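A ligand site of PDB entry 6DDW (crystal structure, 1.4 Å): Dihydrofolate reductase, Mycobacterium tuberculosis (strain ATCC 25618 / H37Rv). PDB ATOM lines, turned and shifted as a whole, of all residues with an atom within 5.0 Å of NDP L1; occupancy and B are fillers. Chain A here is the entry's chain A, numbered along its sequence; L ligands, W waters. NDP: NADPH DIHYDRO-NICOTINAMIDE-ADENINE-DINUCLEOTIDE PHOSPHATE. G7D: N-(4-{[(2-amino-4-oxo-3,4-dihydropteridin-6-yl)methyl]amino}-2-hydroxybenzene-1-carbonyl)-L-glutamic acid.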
ATOM      1  N   ILE A   7     -23.573  34.694  -3.855  1.00  0.00           N
ATOM      2  CA  ILE A   7     -23.341  34.980  -5.268  1.00  0.00           C
ATOM      3  C   ILE A   7     -22.285  34.002  -5.774  1.00  0.00           C
ATOM      4  O   ILE A   7     -21.262  33.782  -5.113  1.00  0.00           O
ATOM      5  CB  ILE A   7     -22.897  36.438  -5.492  1.00  0.00           C
ATOM      6  CG1 ILE A   7     -22.658  36.698  -6.981  1.00  0.00           C
ATOM      7  CG2 ILE A   7     -21.666  36.778  -4.650  1.00  0.00           C
ATOM      8  CD1 ILE A   7     -22.564  38.171  -7.310  1.00  0.00           C
ATOM      9  N   TRP A   8     -22.544  33.380  -6.933  1.00  0.00           N
ATOM     10  CA  TRP A   8     -21.570  32.491  -7.559  1.00  0.00           C
ATOM     11  C   TRP A   8     -21.811  32.372  -9.047  1.00  0.00           C
ATOM     12  O   TRP A   8     -22.878  32.735  -9.529  1.00  0.00           O
ATOM     13  CB  TRP A   8     -21.583  31.093  -6.914  1.00  0.00           C
ATOM     14  CG  TRP A   8     -22.766  30.195  -7.264  1.00  0.00           C
ATOM     15  CD1 TRP A   8     -22.879  29.360  -8.354  1.00  0.00           C
ATOM     16  CD2 TRP A   8     -23.950  29.998  -6.488  1.00  0.00           C
ATOM     17  NE1 TRP A   8     -24.083  28.694  -8.322  1.00  0.00           N
ATOM     18  CE2 TRP A   8     -24.746  29.040  -7.176  1.00  0.00           C
ATOM     19  CE3 TRP A   8     -24.426  30.531  -5.292  1.00  0.00           C
ATOM     20  CZ2 TRP A   8     -25.994  28.627  -6.702  1.00  0.00           C
ATOM     21  CZ3 TRP A   8     -25.666  30.108  -4.817  1.00  0.00           C
ATOM     22  CH2 TRP A   8     -26.424  29.147  -5.525  1.00  0.00           C
ATOM     23  N   ALA A   9     -20.820  31.806  -9.744  1.00  0.00           N
ATOM     24  CA  ALA A   9     -20.945  31.420 -11.139  1.00  0.00           C
ATOM     25  C   ALA A   9     -20.641  29.932 -11.223  1.00  0.00           C
ATOM     26  O   ALA A   9     -19.625  29.461 -10.690  1.00  0.00           O
ATOM     27  CB  ALA A   9     -19.956  32.223 -11.990  1.00  0.00           C
ATOM     28  N   ILE A  16     -17.944  24.836  -9.749  1.00  0.00           N
ATOM     29  CA  ILE A  16     -17.561  26.224  -9.504  1.00  0.00           C
ATOM     30  C   ILE A  16     -16.055  26.422  -9.360  1.00  0.00           C
ATOM     31  O   ILE A  16     -15.557  27.539  -9.483  1.00  0.00           O
ATOM     32  CB  ILE A  16     -18.258  26.851  -8.249  1.00  0.00           C
ATOM     33  CG1 ILE A  16     -17.833  26.145  -6.951  1.00  0.00           C
ATOM     34  CG2 ILE A  16     -19.765  26.837  -8.428  1.00  0.00           C
ATOM     35  CD1 ILE A  16     -18.245  26.886  -5.710  1.00  0.00           C
ATOM     36  N   GLY A  17     -15.330  25.339  -9.088  1.00  0.00           N
ATOM     37  CA  GLY A  17     -13.898  25.417  -8.861  1.00  0.00           C
ATOM     38  C   GLY A  17     -13.196  24.105  -9.145  1.00  0.00           C
ATOM     39  O   GLY A  17     -13.756  23.020  -8.932  1.00  0.00           O
ATOM     40  N   ARG A  18     -11.962  24.209  -9.621  1.00  0.00           N
ATOM     41  CA  ARG A  18     -11.122  23.043  -9.867  1.00  0.00           C
ATOM     42  C   ARG A  18      -9.681  23.519  -9.765  1.00  0.00           C
ATOM     43  O   ARG A  18      -9.348  24.604 -10.247  1.00  0.00           O
ATOM     44  CB  ARG A  18     -11.399  22.472 -11.248  1.00  0.00           C
ATOM     45  CG  ARG A  18     -10.588  21.238 -11.590  1.00  0.00           C
ATOM     46  CD  ARG A  18     -11.062  20.623 -12.915  1.00  0.00           C
ATOM     47  NE  ARG A  18     -12.418  20.099 -12.805  1.00  0.00           N
ATOM     48  CZ  ARG A  18     -13.192  19.788 -13.830  1.00  0.00           C
ATOM     49  NH1 ARG A  18     -12.742  19.942 -15.073  1.00  0.00           N
ATOM     50  NH2 ARG A  18     -14.413  19.317 -13.633  1.00  0.00           N
ATOM     51  N   GLY A  20      -8.060  24.794  -7.435  1.00  0.00           N
ATOM     52  CA  GLY A  20      -7.878  25.989  -6.627  1.00  0.00           C
ATOM     53  C   GLY A  20      -8.208  27.272  -7.353  1.00  0.00           C
ATOM     54  O   GLY A  20      -7.844  28.361  -6.906  1.00  0.00           O
ATOM     55  N   ASP A  21      -8.887  27.146  -8.488  1.00  0.00           N
ATOM     56  CA  ASP A  21      -9.260  28.292  -9.314  1.00  0.00           C
ATOM     57  C   ASP A  21     -10.638  28.081  -9.929  1.00  0.00           C
ATOM     58  O   ASP A  21     -11.305  27.082  -9.652  1.00  0.00           O
ATOM     59  CB  ASP A  21      -8.234  28.481 -10.422  1.00  0.00           C
ATOM     60  CG  ASP A  21      -6.908  28.982  -9.917  1.00  0.00           C
ATOM     61  OD1 ASP A  21      -6.891  29.987  -9.163  1.00  0.00           O
ATOM     62  OD2 ASP A  21      -5.873  28.366 -10.266  1.00  0.00           O
ATOM     63  N   ILE A  22     -11.057  29.026 -10.750  1.00  0.00           N
ATOM     64  CA  ILE A  22     -12.310  28.943 -11.473  1.00  0.00           C
ATOM     65  C   ILE A  22     -11.970  28.542 -12.896  1.00  0.00           C
ATOM     66  O   ILE A  22     -11.212  29.228 -13.566  1.00  0.00           O
ATOM     67  CB  ILE A  22     -13.045  30.293 -11.439  1.00  0.00           C
ATOM     68  CG1 ILE A  22     -13.450  30.618  -9.997  1.00  0.00           C
ATOM     69  CG2 ILE A  22     -14.268  30.254 -12.337  1.00  0.00           C
ATOM     70  CD1 ILE A  22     -14.139  31.967  -9.798  1.00  0.00           C
ATOM     71  N   TRP A  24     -12.776  28.745 -15.962  1.00  0.00           N
ATOM     72  CA  TRP A  24     -13.186  29.441 -17.173  1.00  0.00           C
ATOM     73  C   TRP A  24     -12.880  30.916 -17.036  1.00  0.00           C
ATOM     74  O   TRP A  24     -12.502  31.381 -15.959  1.00  0.00           O
ATOM     75  CB  TRP A  24     -14.679  29.269 -17.447  1.00  0.00           C
ATOM     76  CG  TRP A  24     -15.536  29.774 -16.320  1.00  0.00           C
ATOM     77  CD1 TRP A  24     -15.821  31.067 -16.015  1.00  0.00           C
ATOM     78  CD2 TRP A  24     -16.218  28.971 -15.355  1.00  0.00           C
ATOM     79  NE1 TRP A  24     -16.633  31.133 -14.901  1.00  0.00           N
ATOM     80  CE2 TRP A  24     -16.892  29.862 -14.478  1.00  0.00           C
ATOM     81  CE3 TRP A  24     -16.321  27.604 -15.129  1.00  0.00           C
ATOM     82  CZ2 TRP A  24     -17.655  29.412 -13.409  1.00  0.00           C
ATOM     83  CZ3 TRP A  24     -17.081  27.156 -14.070  1.00  0.00           C
ATOM     84  CH2 TRP A  24     -17.735  28.059 -13.216  1.00  0.00           C
ATOM     85  N   GLY A  45     -14.596  31.616   2.436  1.00  0.00           N
ATOM     86  CA  GLY A  45     -13.697  30.636   3.018  1.00  0.00           C
ATOM     87  C   GLY A  45     -12.248  30.982   2.750  1.00  0.00           C
ATOM     88  O   GLY A  45     -11.919  31.695   1.791  1.00  0.00           O
ATOM     89  N   ARG A  46     -11.365  30.494   3.609  1.00  0.00           N
ATOM     90  CA  ARG A  46      -9.938  30.775   3.472  1.00  0.00           C
ATOM     91  C   ARG A  46      -9.373  30.401   2.097  1.00  0.00           C
ATOM     92  O   ARG A  46      -8.538  31.102   1.541  1.00  0.00           O
ATOM     93  CB  ARG A  46      -9.159  30.099   4.607  1.00  0.00           C
ATOM     94  CG  ARG A  46      -7.723  30.557   4.748  1.00  0.00           C
ATOM     95  CD  ARG A  46      -6.784  29.684   3.930  1.00  0.00           C
ATOM     96  NE  ARG A  46      -6.907  28.289   4.305  1.00  0.00           N
ATOM     97  CZ  ARG A  46      -6.436  27.272   3.584  1.00  0.00           C
ATOM     98  NH1 ARG A  46      -5.788  27.505   2.453  1.00  0.00           N
ATOM     99  NH2 ARG A  46      -6.595  26.026   4.013  1.00  0.00           N
ATOM    100  N   ARG A  47      -9.831  29.283   1.518  1.00  0.00           N
ATOM    101  CA  ARG A  47      -9.331  28.928   0.198  1.00  0.00           C
ATOM    102  C   ARG A  47      -9.714  29.950  -0.865  1.00  0.00           C
ATOM    103  O   ARG A  47      -8.922  30.261  -1.744  1.00  0.00           O
ATOM    104  CB  ARG A  47      -9.828  27.539  -0.203  1.00  0.00           C
ATOM    105  CG  ARG A  47      -9.143  26.426   0.532  1.00  0.00           C
ATOM    106  CD  ARG A  47      -9.717  25.109   0.052  1.00  0.00           C
ATOM    107  NE  ARG A  47      -9.050  23.984   0.661  1.00  0.00           N
ATOM    108  CZ  ARG A  47      -9.547  22.749   0.658  1.00  0.00           C
ATOM    109  NH1 ARG A  47     -10.731  22.517   0.094  1.00  0.00           N
ATOM    110  NH2 ARG A  47      -8.871  21.755   1.227  1.00  0.00           N
ATOM    111  N   THR A  48     -10.929  30.463  -0.775  1.00  0.00           N
ATOM    112  CA  THR A  48     -11.379  31.464  -1.736  1.00  0.00           C
ATOM    113  C   THR A  48     -10.585  32.754  -1.582  1.00  0.00           C
ATOM    114  O   THR A  48     -10.204  33.371  -2.571  1.00  0.00           O
ATOM    115  CB  THR A  48     -12.903  31.677  -1.660  1.00  0.00           C
ATOM    116  OG1 THR A  48     -13.547  30.499  -2.162  1.00  0.00           O
ATOM    117  CG2 THR A  48     -13.351  32.857  -2.495  1.00  0.00           C
ATOM    118  N   SER A  51      -7.469  32.324  -3.314  1.00  0.00           N
ATOM    119  CA  SER A  51      -7.619  32.276  -4.770  1.00  0.00           C
ATOM    120  C   SER A  51      -7.726  33.662  -5.415  1.00  0.00           C
ATOM    121  O   SER A  51      -7.621  33.791  -6.629  1.00  0.00           O
ATOM    122  CB  SER A  51      -8.836  31.430  -5.145  1.00  0.00           C
ATOM    123  OG  SER A  51     -10.037  32.147  -4.953  1.00  0.00           O
ATOM    124  N   LEU A  67     -13.322  33.158   6.720  1.00  0.00           N
ATOM    125  CA  LEU A  67     -13.509  32.072   7.677  1.00  0.00           C
ATOM    126  C   LEU A  67     -12.331  31.111   7.631  1.00  0.00           C
ATOM    127  O   LEU A  67     -11.985  30.601   6.566  1.00  0.00           O
ATOM    128  CB  LEU A  67     -14.759  31.282   7.311  1.00  0.00           C
ATOM    129  CG  LEU A  67     -16.116  31.703   7.840  1.00  0.00           C
ATOM    130  CD1 LEU A  67     -17.179  30.776   7.248  1.00  0.00           C
ATOM    131  CD2 LEU A  67     -16.160  31.600   9.367  1.00  0.00           C
ATOM    132  N   SER A  68     -11.742  30.863   8.792  1.00  0.00           N
ATOM    133  CA  SER A  68     -10.661  29.881   8.912  1.00  0.00           C
ATOM    134  C   SER A  68     -10.719  29.232  10.293  1.00  0.00           C
ATOM    135  O   SER A  68     -11.115  29.873  11.266  1.00  0.00           O
ATOM    136  CB  SER A  68      -9.309  30.550   8.706  1.00  0.00           C
ATOM    137  OG  SER A  68      -8.245  29.661   8.985  1.00  0.00           O
ATOM    138  N   ARG A  69     -10.341  27.965  10.376  1.00  0.00           N
ATOM    139  CA  ARG A  69     -10.236  27.309  11.672  1.00  0.00           C
ATOM    140  C   ARG A  69      -8.841  27.488  12.277  1.00  0.00           C
ATOM    141  O   ARG A  69      -8.598  27.093  13.415  1.00  0.00           O
ATOM    142  CB  ARG A  69     -10.563  25.823  11.558  1.00  0.00           C
ATOM    143  CG  ARG A  69     -12.018  25.529  11.245  1.00  0.00           C
ATOM    144  CD  ARG A  69     -12.264  24.036  11.392  1.00  0.00           C
ATOM    145  NE  ARG A  69     -13.619  23.618  11.008  1.00  0.00           N
ATOM    146  CZ  ARG A  69     -13.943  23.262   9.764  1.00  0.00           C
ATOM    147  NH1 ARG A  69     -13.024  23.279   8.816  1.00  0.00           N
ATOM    148  NH2 ARG A  69     -15.185  22.883   9.498  1.00  0.00           N
ATOM    149  N   GLN A  70      -7.925  28.086  11.518  1.00  0.00           N
ATOM    150  CA  GLN A  70      -6.622  28.453  12.036  1.00  0.00           C
ATOM    151  C   GLN A  70      -6.777  29.724  12.883  1.00  0.00           C
ATOM    152  O   GLN A  70      -7.027  30.800  12.342  1.00  0.00           O
ATOM    153  CB  GLN A  70      -5.610  28.700  10.911  1.00  0.00           C
ATOM    154  CG  GLN A  70      -5.593  27.628   9.816  1.00  0.00           C
ATOM    155  CD  GLN A  70      -4.668  27.986   8.670  1.00  0.00           C
ATOM    156  OE1 GLN A  70      -3.555  28.470   8.876  1.00  0.00           O
ATOM    157  NE2 GLN A  70      -5.126  27.754   7.432  1.00  0.00           N
ATOM    158  N   GLY A  82     -13.522  32.725  13.103  1.00  0.00           N
ATOM    159  CA  GLY A  82     -13.477  31.275  13.270  1.00  0.00           C
ATOM    160  C   GLY A  82     -14.811  30.580  13.147  1.00  0.00           C
ATOM    161  O   GLY A  82     -14.884  29.344  13.222  1.00  0.00           O
ATOM    162  N   SER A  83     -15.878  31.345  12.964  1.00  0.00           N
ATOM    163  CA  SER A  83     -17.213  30.771  12.861  1.00  0.00           C
ATOM    164  C   SER A  83     -18.098  31.611  11.951  1.00  0.00           C
ATOM    165  O   SER A  83     -17.878  32.821  11.793  1.00  0.00           O
ATOM    166  CB  SER A  83     -17.854  30.677  14.252  1.00  0.00           C
ATOM    167  OG  SER A  83     -18.109  31.963  14.768  1.00  0.00           O
ATOM    168  N   ILE A  96     -19.377  34.849  -0.797  1.00  0.00           N
ATOM    169  CA  ILE A  96     -18.764  34.732  -2.104  1.00  0.00           C
ATOM    170  C   ILE A  96     -17.932  33.449  -2.233  1.00  0.00           C
ATOM    171  O   ILE A  96     -17.018  33.368  -3.059  1.00  0.00           O
ATOM    172  CB  ILE A  96     -17.904  35.977  -2.414  1.00  0.00           C
ATOM    173  CG1 ILE A  96     -16.659  36.039  -1.538  1.00  0.00           C
ATOM    174  CG2 ILE A  96     -18.751  37.251  -2.281  1.00  0.00           C
ATOM    175  CD1 ILE A  96     -15.515  36.831  -2.167  1.00  0.00           C
ATOM    176  N   GLY A  97     -18.290  32.443  -1.427  1.00  0.00           N
ATOM    177  CA  GLY A  97     -17.750  31.097  -1.622  1.00  0.00           C
ATOM    178  C   GLY A  97     -16.687  30.678  -0.638  1.00  0.00           C
ATOM    179  O   GLY A  97     -16.434  31.427   0.315  1.00  0.00           O
ATOM    180  N   GLY A  98     -16.070  29.503  -0.823  1.00  0.00           N
ATOM    181  CA  GLY A  98     -16.298  28.647  -1.976  1.00  0.00           C
ATOM    182  C   GLY A  98     -17.294  27.522  -1.692  1.00  0.00           C
ATOM    183  O   GLY A  98     -18.295  27.755  -1.030  1.00  0.00           O
ATOM    184  N   GLY A  99     -17.049  26.323  -2.218  1.00  0.00           N
ATOM    185  CA  GLY A  99     -17.999  25.232  -2.030  1.00  0.00           C
ATOM    186  C   GLY A  99     -18.382  24.974  -0.589  1.00  0.00           C
ATOM    187  O   GLY A  99     -19.568  24.857  -0.281  1.00  0.00           O
ATOM    188  N   GLN A 100     -17.392  24.900   0.287  1.00  0.00           N
ATOM    189  CA  GLN A 100     -17.683  24.643   1.705  1.00  0.00           C
ATOM    190  C   GLN A 100     -18.514  25.779   2.324  1.00  0.00           C
ATOM    191  O   GLN A 100     -19.520  25.534   3.003  1.00  0.00           O
ATOM    192  CB  GLN A 100     -16.395  24.480   2.486  1.00  0.00           C
ATOM    193  CG  GLN A 100     -15.581  23.254   2.104  1.00  0.00           C
ATOM    194  CD  GLN A 100     -14.285  23.189   2.860  1.00  0.00           C
ATOM    195  OE1 GLN A 100     -14.213  23.634   4.012  1.00  0.00           O
ATOM    196  NE2 GLN A 100     -13.252  22.655   2.225  1.00  0.00           N
ATOM    197  N   VAL A 101     -18.114  27.017   2.049  1.00  0.00           N
ATOM    198  CA  VAL A 101     -18.777  28.116   2.719  1.00  0.00           C
ATOM    199  C   VAL A 101     -20.167  28.409   2.127  1.00  0.00           C
ATOM    200  O   VAL A 101     -21.077  28.786   2.875  1.00  0.00           O
ATOM    201  CB  VAL A 101     -17.874  29.354   2.795  1.00  0.00           C
ATOM    202  CG1 VAL A 101     -18.651  30.576   3.263  1.00  0.00           C
ATOM    203  CG2 VAL A 101     -16.706  29.062   3.738  1.00  0.00           C
ATOM    204  N   TYR A 102     -20.362  28.179   0.830  1.00  0.00           N
ATOM    205  CA  TYR A 102     -21.725  28.281   0.292  1.00  0.00           C
ATOM    206  C   TYR A 102     -22.647  27.293   0.996  1.00  0.00           C
ATOM    207  O   TYR A 102     -23.786  27.633   1.308  1.00  0.00           O
ATOM    208  CB  TYR A 102     -21.767  28.021  -1.216  1.00  0.00           C
ATOM    209  CG  TYR A 102     -21.165  29.090  -2.111  1.00  0.00           C
ATOM    210  CD1 TYR A 102     -21.462  30.442  -1.972  1.00  0.00           C
ATOM    211  CD2 TYR A 102     -20.298  28.718  -3.139  1.00  0.00           C
ATOM    212  CE1 TYR A 102     -20.924  31.395  -2.812  1.00  0.00           C
ATOM    213  CE2 TYR A 102     -19.752  29.660  -3.978  1.00  0.00           C
ATOM    214  CZ  TYR A 102     -20.063  30.996  -3.803  1.00  0.00           C
ATOM    215  OH  TYR A 102     -19.500  31.924  -4.639  1.00  0.00           O
ATOM    216  N   LEU A 104     -22.330  25.975   3.975  1.00  0.00           N
ATOM    217  CA  LEU A 104     -22.462  26.392   5.364  1.00  0.00           C
ATOM    218  C   LEU A 104     -23.476  27.519   5.482  1.00  0.00           C
ATOM    219  O   LEU A 104     -24.273  27.566   6.428  1.00  0.00           O
ATOM    220  CB  LEU A 104     -21.088  26.881   5.841  1.00  0.00           C
ATOM    221  CG  LEU A 104     -20.782  27.053   7.327  1.00  0.00           C
ATOM    222  CD1 LEU A 104     -20.837  25.687   7.995  1.00  0.00           C
ATOM    223  CD2 LEU A 104     -19.404  27.676   7.463  1.00  0.00           C
ATOM    224  N   ALA A 128     -14.899  21.859  -6.483  1.00  0.00           N
ATOM    225  CA  ALA A 128     -15.833  22.616  -5.661  1.00  0.00           C
ATOM    226  C   ALA A 128     -17.125  22.749  -6.448  1.00  0.00           C
ATOM    227  O   ALA A 128     -17.089  23.036  -7.670  1.00  0.00           O
ATOM    228  CB  ALA A 128     -15.267  23.986  -5.325  1.00  0.00           C
HETATM  229  PA  NDP L   1     -13.668  27.533   0.671  1.00  0.00           P
HETATM  230  O1A NDP L   1     -15.076  27.260   0.997  1.00  0.00           O
HETATM  231  O2A NDP L   1     -13.313  28.730  -0.159  1.00  0.00           O
HETATM  232  O5B NDP L   1     -12.724  27.636   2.009  1.00  0.00           O
HETATM  233  C5B NDP L   1     -12.807  26.465   2.806  1.00  0.00           C
HETATM  234  C4B NDP L   1     -12.016  26.835   4.071  1.00  0.00           C
HETATM  235  O4B NDP L   1     -12.829  27.672   4.871  1.00  0.00           O
HETATM  236  C3B NDP L   1     -11.609  25.631   4.953  1.00  0.00           C
HETATM  237  O3B NDP L   1     -10.403  25.062   4.499  1.00  0.00           O
HETATM  238  C2B NDP L   1     -11.374  26.393   6.297  1.00  0.00           C
HETATM  239  O2B NDP L   1     -10.349  27.247   6.288  1.00  0.00           O
HETATM  240  C1B NDP L   1     -12.603  27.349   6.261  1.00  0.00           C
HETATM  241  N9A NDP L   1     -13.795  26.785   6.826  1.00  0.00           N
HETATM  242  C8A NDP L   1     -14.692  25.868   6.260  1.00  0.00           C
HETATM  243  N7A NDP L   1     -15.709  25.546   7.061  1.00  0.00           N
HETATM  244  C5A NDP L   1     -15.447  26.289   8.229  1.00  0.00           C
HETATM  245  C6A NDP L   1     -16.131  26.395   9.446  1.00  0.00           C
HETATM  246  N6A NDP L   1     -17.295  25.683   9.666  1.00  0.00           N
HETATM  247  N1A NDP L   1     -15.658  27.217  10.432  1.00  0.00           N
HETATM  248  C2A NDP L   1     -14.496  27.891  10.152  1.00  0.00           C
HETATM  249  N3A NDP L   1     -13.735  27.895   9.042  1.00  0.00           N
HETATM  250  C4A NDP L   1     -14.250  27.063   8.084  1.00  0.00           C
HETATM  251  O3  NDP L   1     -12.935  26.165  -0.007  1.00  0.00           O
HETATM  252  PN  NDP L   1     -13.530  25.280  -1.235  1.00  0.00           P
HETATM  253  O1N NDP L   1     -12.374  24.429  -1.591  1.00  0.00           O
HETATM  254  O2N NDP L   1     -14.902  24.722  -0.954  1.00  0.00           O
HETATM  255  O5D NDP L   1     -13.847  26.358  -2.513  1.00  0.00           O
HETATM  256  C5D NDP L   1     -12.699  26.899  -3.128  1.00  0.00           C
HETATM  257  C4D NDP L   1     -12.913  26.770  -4.640  1.00  0.00           C
HETATM  258  O4D NDP L   1     -14.107  27.461  -5.059  1.00  0.00           O
HETATM  259  C3D NDP L   1     -11.735  27.378  -5.448  1.00  0.00           C
HETATM  260  O3D NDP L   1     -11.514  26.535  -6.556  1.00  0.00           O
HETATM  261  C2D NDP L   1     -12.302  28.733  -5.901  1.00  0.00           C
HETATM  262  O2D NDP L   1     -11.739  29.221  -7.095  1.00  0.00           O
HETATM  263  C1D NDP L   1     -13.767  28.316  -6.162  1.00  0.00           C
HETATM  264  N1N NDP L   1     -14.702  29.448  -6.124  1.00  0.00           N
HETATM  265  C2N NDP L   1     -15.543  29.644  -7.196  1.00  0.00           C
HETATM  266  C3N NDP L   1     -16.505  30.596  -7.164  1.00  0.00           C
HETATM  267  C7N NDP L   1     -17.389  30.768  -8.287  1.00  0.00           C
HETATM  268  O7N NDP L   1     -18.375  31.534  -8.240  1.00  0.00           O
HETATM  269  N7N NDP L   1     -17.137  30.078  -9.456  1.00  0.00           N
HETATM  270  C4N NDP L   1     -16.704  31.465  -6.003  1.00  0.00           C
HETATM  271  C5N NDP L   1     -15.740  31.192  -4.901  1.00  0.00           C
HETATM  272  C6N NDP L   1     -14.806  30.253  -4.972  1.00  0.00           C
HETATM  273  P2B NDP L   1      -8.815  26.687   7.055  1.00  0.00           P
HETATM  274  O1X NDP L   1      -8.525  25.544   6.136  1.00  0.00           O
HETATM  275  O2X NDP L   1      -7.902  27.903   6.939  1.00  0.00           O
HETATM  276  O3X NDP L   1      -9.295  26.334   8.427  1.00  0.00           O
HETATM  277  C4  G7D L   2     -17.281  34.899 -10.073  1.00  0.00           C
HETATM  278  C6  G7D L   2     -15.775  34.495  -6.825  1.00  0.00           C
HETATM  279  C7  G7D L   2     -16.893  34.601  -6.010  1.00  0.00           C
HETATM  280  C9  G7D L   2     -14.535  34.264  -6.221  1.00  0.00           C
HETATM  281  N1  G7D L   2     -19.471  35.135  -8.402  1.00  0.00           N
HETATM  282  N2  G7D L   2     -20.837  35.476 -10.248  1.00  0.00           N
HETATM  283  N3  G7D L   2     -18.544  35.138 -10.598  1.00  0.00           N
HETATM  284  OE1 G7D L   2     -14.873  43.933 -13.060  1.00  0.00           O
HETATM  285  CD  G7D L   2     -14.164  43.024 -12.573  1.00  0.00           C
HETATM  286  OE2 G7D L   2     -13.362  42.310 -13.208  1.00  0.00           O
HETATM  287  CG  G7D L   2     -14.269  42.769 -11.060  1.00  0.00           C
HETATM  288  CB  G7D L   2     -12.859  42.518 -10.540  1.00  0.00           C
HETATM  289  CA  G7D L   2     -12.831  42.173  -9.039  1.00  0.00           C
HETATM  290  C   G7D L   2     -13.798  43.021  -8.182  1.00  0.00           C
HETATM  291  OXT G7D L   2     -13.478  44.203  -7.948  1.00  0.00           O
HETATM  292  O   G7D L   2     -14.813  42.440  -7.720  1.00  0.00           O
HETATM  293  N   G7D L   2     -13.080  40.746  -8.765  1.00  0.00           N
HETATM  294  CAT G7D L   2     -12.177  39.778  -8.969  1.00  0.00           C
HETATM  295  OAU G7D L   2     -11.089  40.011  -9.505  1.00  0.00           O
HETATM  296  CAR G7D L   2     -12.505  38.490  -8.508  1.00  0.00           C
HETATM  297  CAN G7D L   2     -11.676  37.394  -8.736  1.00  0.00           C
HETATM  298  CAO G7D L   2     -11.980  36.130  -8.263  1.00  0.00           C
HETATM  299  OAS G7D L   2     -10.559  37.649  -9.494  1.00  0.00           O
HETATM  300  CAQ G7D L   2     -13.645  38.263  -7.722  1.00  0.00           C
HETATM  301  CAP G7D L   2     -13.966  36.999  -7.233  1.00  0.00           C
HETATM  302  CAM G7D L   2     -13.135  35.901  -7.504  1.00  0.00           C
HETATM  303  N10 G7D L   2     -13.393  34.658  -7.065  1.00  0.00           N
HETATM  304  N5  G7D L   2     -15.922  34.585  -8.151  1.00  0.00           N
HETATM  305  C4A G7D L   2     -17.130  34.808  -8.692  1.00  0.00           C
HETATM  306  O4  G7D L   2     -16.316  34.788 -10.844  1.00  0.00           O
HETATM  307  C2  G7D L   2     -19.636  35.238  -9.732  1.00  0.00           C
HETATM  308  C8A G7D L   2     -18.264  34.919  -7.892  1.00  0.00           C
HETATM  309  N8  G7D L   2     -18.154  34.813  -6.560  1.00  0.00           N
HETATM  310  O   HOH W   1      -7.227  23.229   6.574  1.00  0.00           O
HETATM  311  O   HOH W   2     -10.877  22.405   3.869  1.00  0.00           O
HETATM  312  O   HOH W   3     -16.355  26.890  13.005  1.00  0.00           O
HETATM  313  O   HOH W   4      -7.272  24.909   9.881  1.00  0.00           O
HETATM  314  O   HOH W   5     -10.127  23.766   8.663  1.00  0.00           O
HETATM  315  O   HOH W   6     -17.521  23.483   6.525  1.00  0.00           O
HETATM  316  O   HOH W   7     -11.850  31.931  -6.963  1.00  0.00           O
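An oxygen (O2A) of NDP L1 lies within hydrogen-bond range of the side-chain hydroxyl of Thr 48 (2.7 Å).
An oxygen (O3D) of NDP L1 sits at hydrogen-bond distance from the backbone carbonyl oxygen (O) of Asp 21.
The backbone NH of Arg 69 is in hydrogen-bond range of an oxygen (O3X) of NDP L1 (2.7 Å).
O2X of NDP L1 sits at hydrogen-bond distance from NE2 of Gln 70 (2.8 Å).
N of Arg 47 is in hydrogen-bond range of O5B of NDP L1.
O3D of NDP L1 is in hydrogen-bond range of N of Asp 21 (3.3 Å).
The backbone NH (N) of Thr 48 is in hydrogen-bond range of an oxygen (O2A) of NDP L1 (3.0 Å).
NH1 of Arg 47 is in salt-bridge range of O1N of NDP L1.
N7N of NDP L1 lies within hydrogen-bond range of O of Ile 16, 3.0 Å away.
A nitrogen (N2) of G7D L2 lies close to the backbone carbonyl oxygen (O) of Trp 8 (3.5 Å).
The guanidinium group of Arg 46 lies within salt-bridge range of an oxygen (O2X) of NDP L1 (2.8 Å).
The backbone carbonyl oxygen of Ala 9 lies within hydrogen-bond range of a nitrogen (N7N) of NDP L1 (2.8 Å).
N of Ala 9 is in hydrogen-bond range of O7N of NDP L1 (2.9 Å).
The backbone NH of Arg 46 is in hydrogen-bond range of an oxygen (O4B) of NDP L1 (3.4 Å).
An oxygen (O2A) of NDP L1 lies within hydrogen-bond range of the backbone NH (N) of Gly 98, at 2.9 Å.
An oxygen (O1A) of NDP L1 is in hydrogen-bond range of the backbone NH (N) of Val 101 (3.2 Å).
The backbone NH of Gln 100 sits at hydrogen-bond distance from an oxygen (O2N) of NDP L1.
N of Gly 99 is in hydrogen-bond range of O2N of NDP L1 (3.0 Å).
OG of Ser 68 lies within hydrogen-bond range of O2X of NDP L1 (2.7 Å).
The backbone NH of Gly 45 is in hydrogen-bond range of the backbone carbonyl oxygen of Gly 97.
N of Arg 46 lies within hydrogen-bond range of O of Leu 67, 3.0 Å away.
NH1 of Arg 47 sits close to NE2 of Gln 100.
O of Ile 7 lies within hydrogen-bond range of OH of Tyr 102 (2.6 Å).
The backbone carbonyl oxygen of Ala 128 lies within hydrogen-bond range of the backbone NH of Ile 16 (2.9 Å).
O of Gly 17 is in hydrogen-bond range of N of Ala 128 (2.9 Å).
The side-chain hydroxyl of Ser 68 lies within hydrogen-bond range of the backbone NH of Gln 70, 3.0 Å away.
The side-chain hydroxyl of Ser 51 lies within hydrogen-bond range of the backbone carbonyl oxygen of Thr 48, 2.7 Å away.
O of Leu 67 sits close to O4B of NDP L1, 3.5 Å away.
Merely in contact with NDP L1: Ile 96 (3.1 Å), Tyr 102 (3.1 Å), Gly 45 (3.3 Å), Trp 8 (3.4 Å), Gly 82 (3.4 Å), Gly 20 (3.5 Å), Gly 17 (3.5 Å), Ile 22 (3.6 Å), Leu 104 (3.6 Å), Ala 128 (3.7 Å), Gly 97 (3.8 Å) and Arg 18 (3.9 Å).
Hydrophobic or aromatic side chains within 4 Å of NDP L1: Trp 8, Ile 16, Ile 22, Leu 67, Val 101, Leu 104 and Ala 128.
Of the 30 residues printed, 26 come within 4 Å of NDP L1.
Water W3 lies within hydrogen-bond range of a nitrogen (N1A) of NDP L1 (2.7 Å) and the backbone carbonyl oxygen (O) of Gly 82 (2.9 Å).
Water W5 lies within hydrogen-bond range of O3X of NDP L1 (2.7 Å) and NH1 of Arg 69 (2.9 Å).
Water W7 lies within hydrogen-bond range of O2D of NDP L1, OG of Ser 51 and N10 of G7D L2.
Water W2 lies within hydrogen-bond range of O3B of NDP L1 (2.8 Å), NE2 of Gln 100 (2.9 Å) and NH2 of Arg 47 (3.4 Å).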
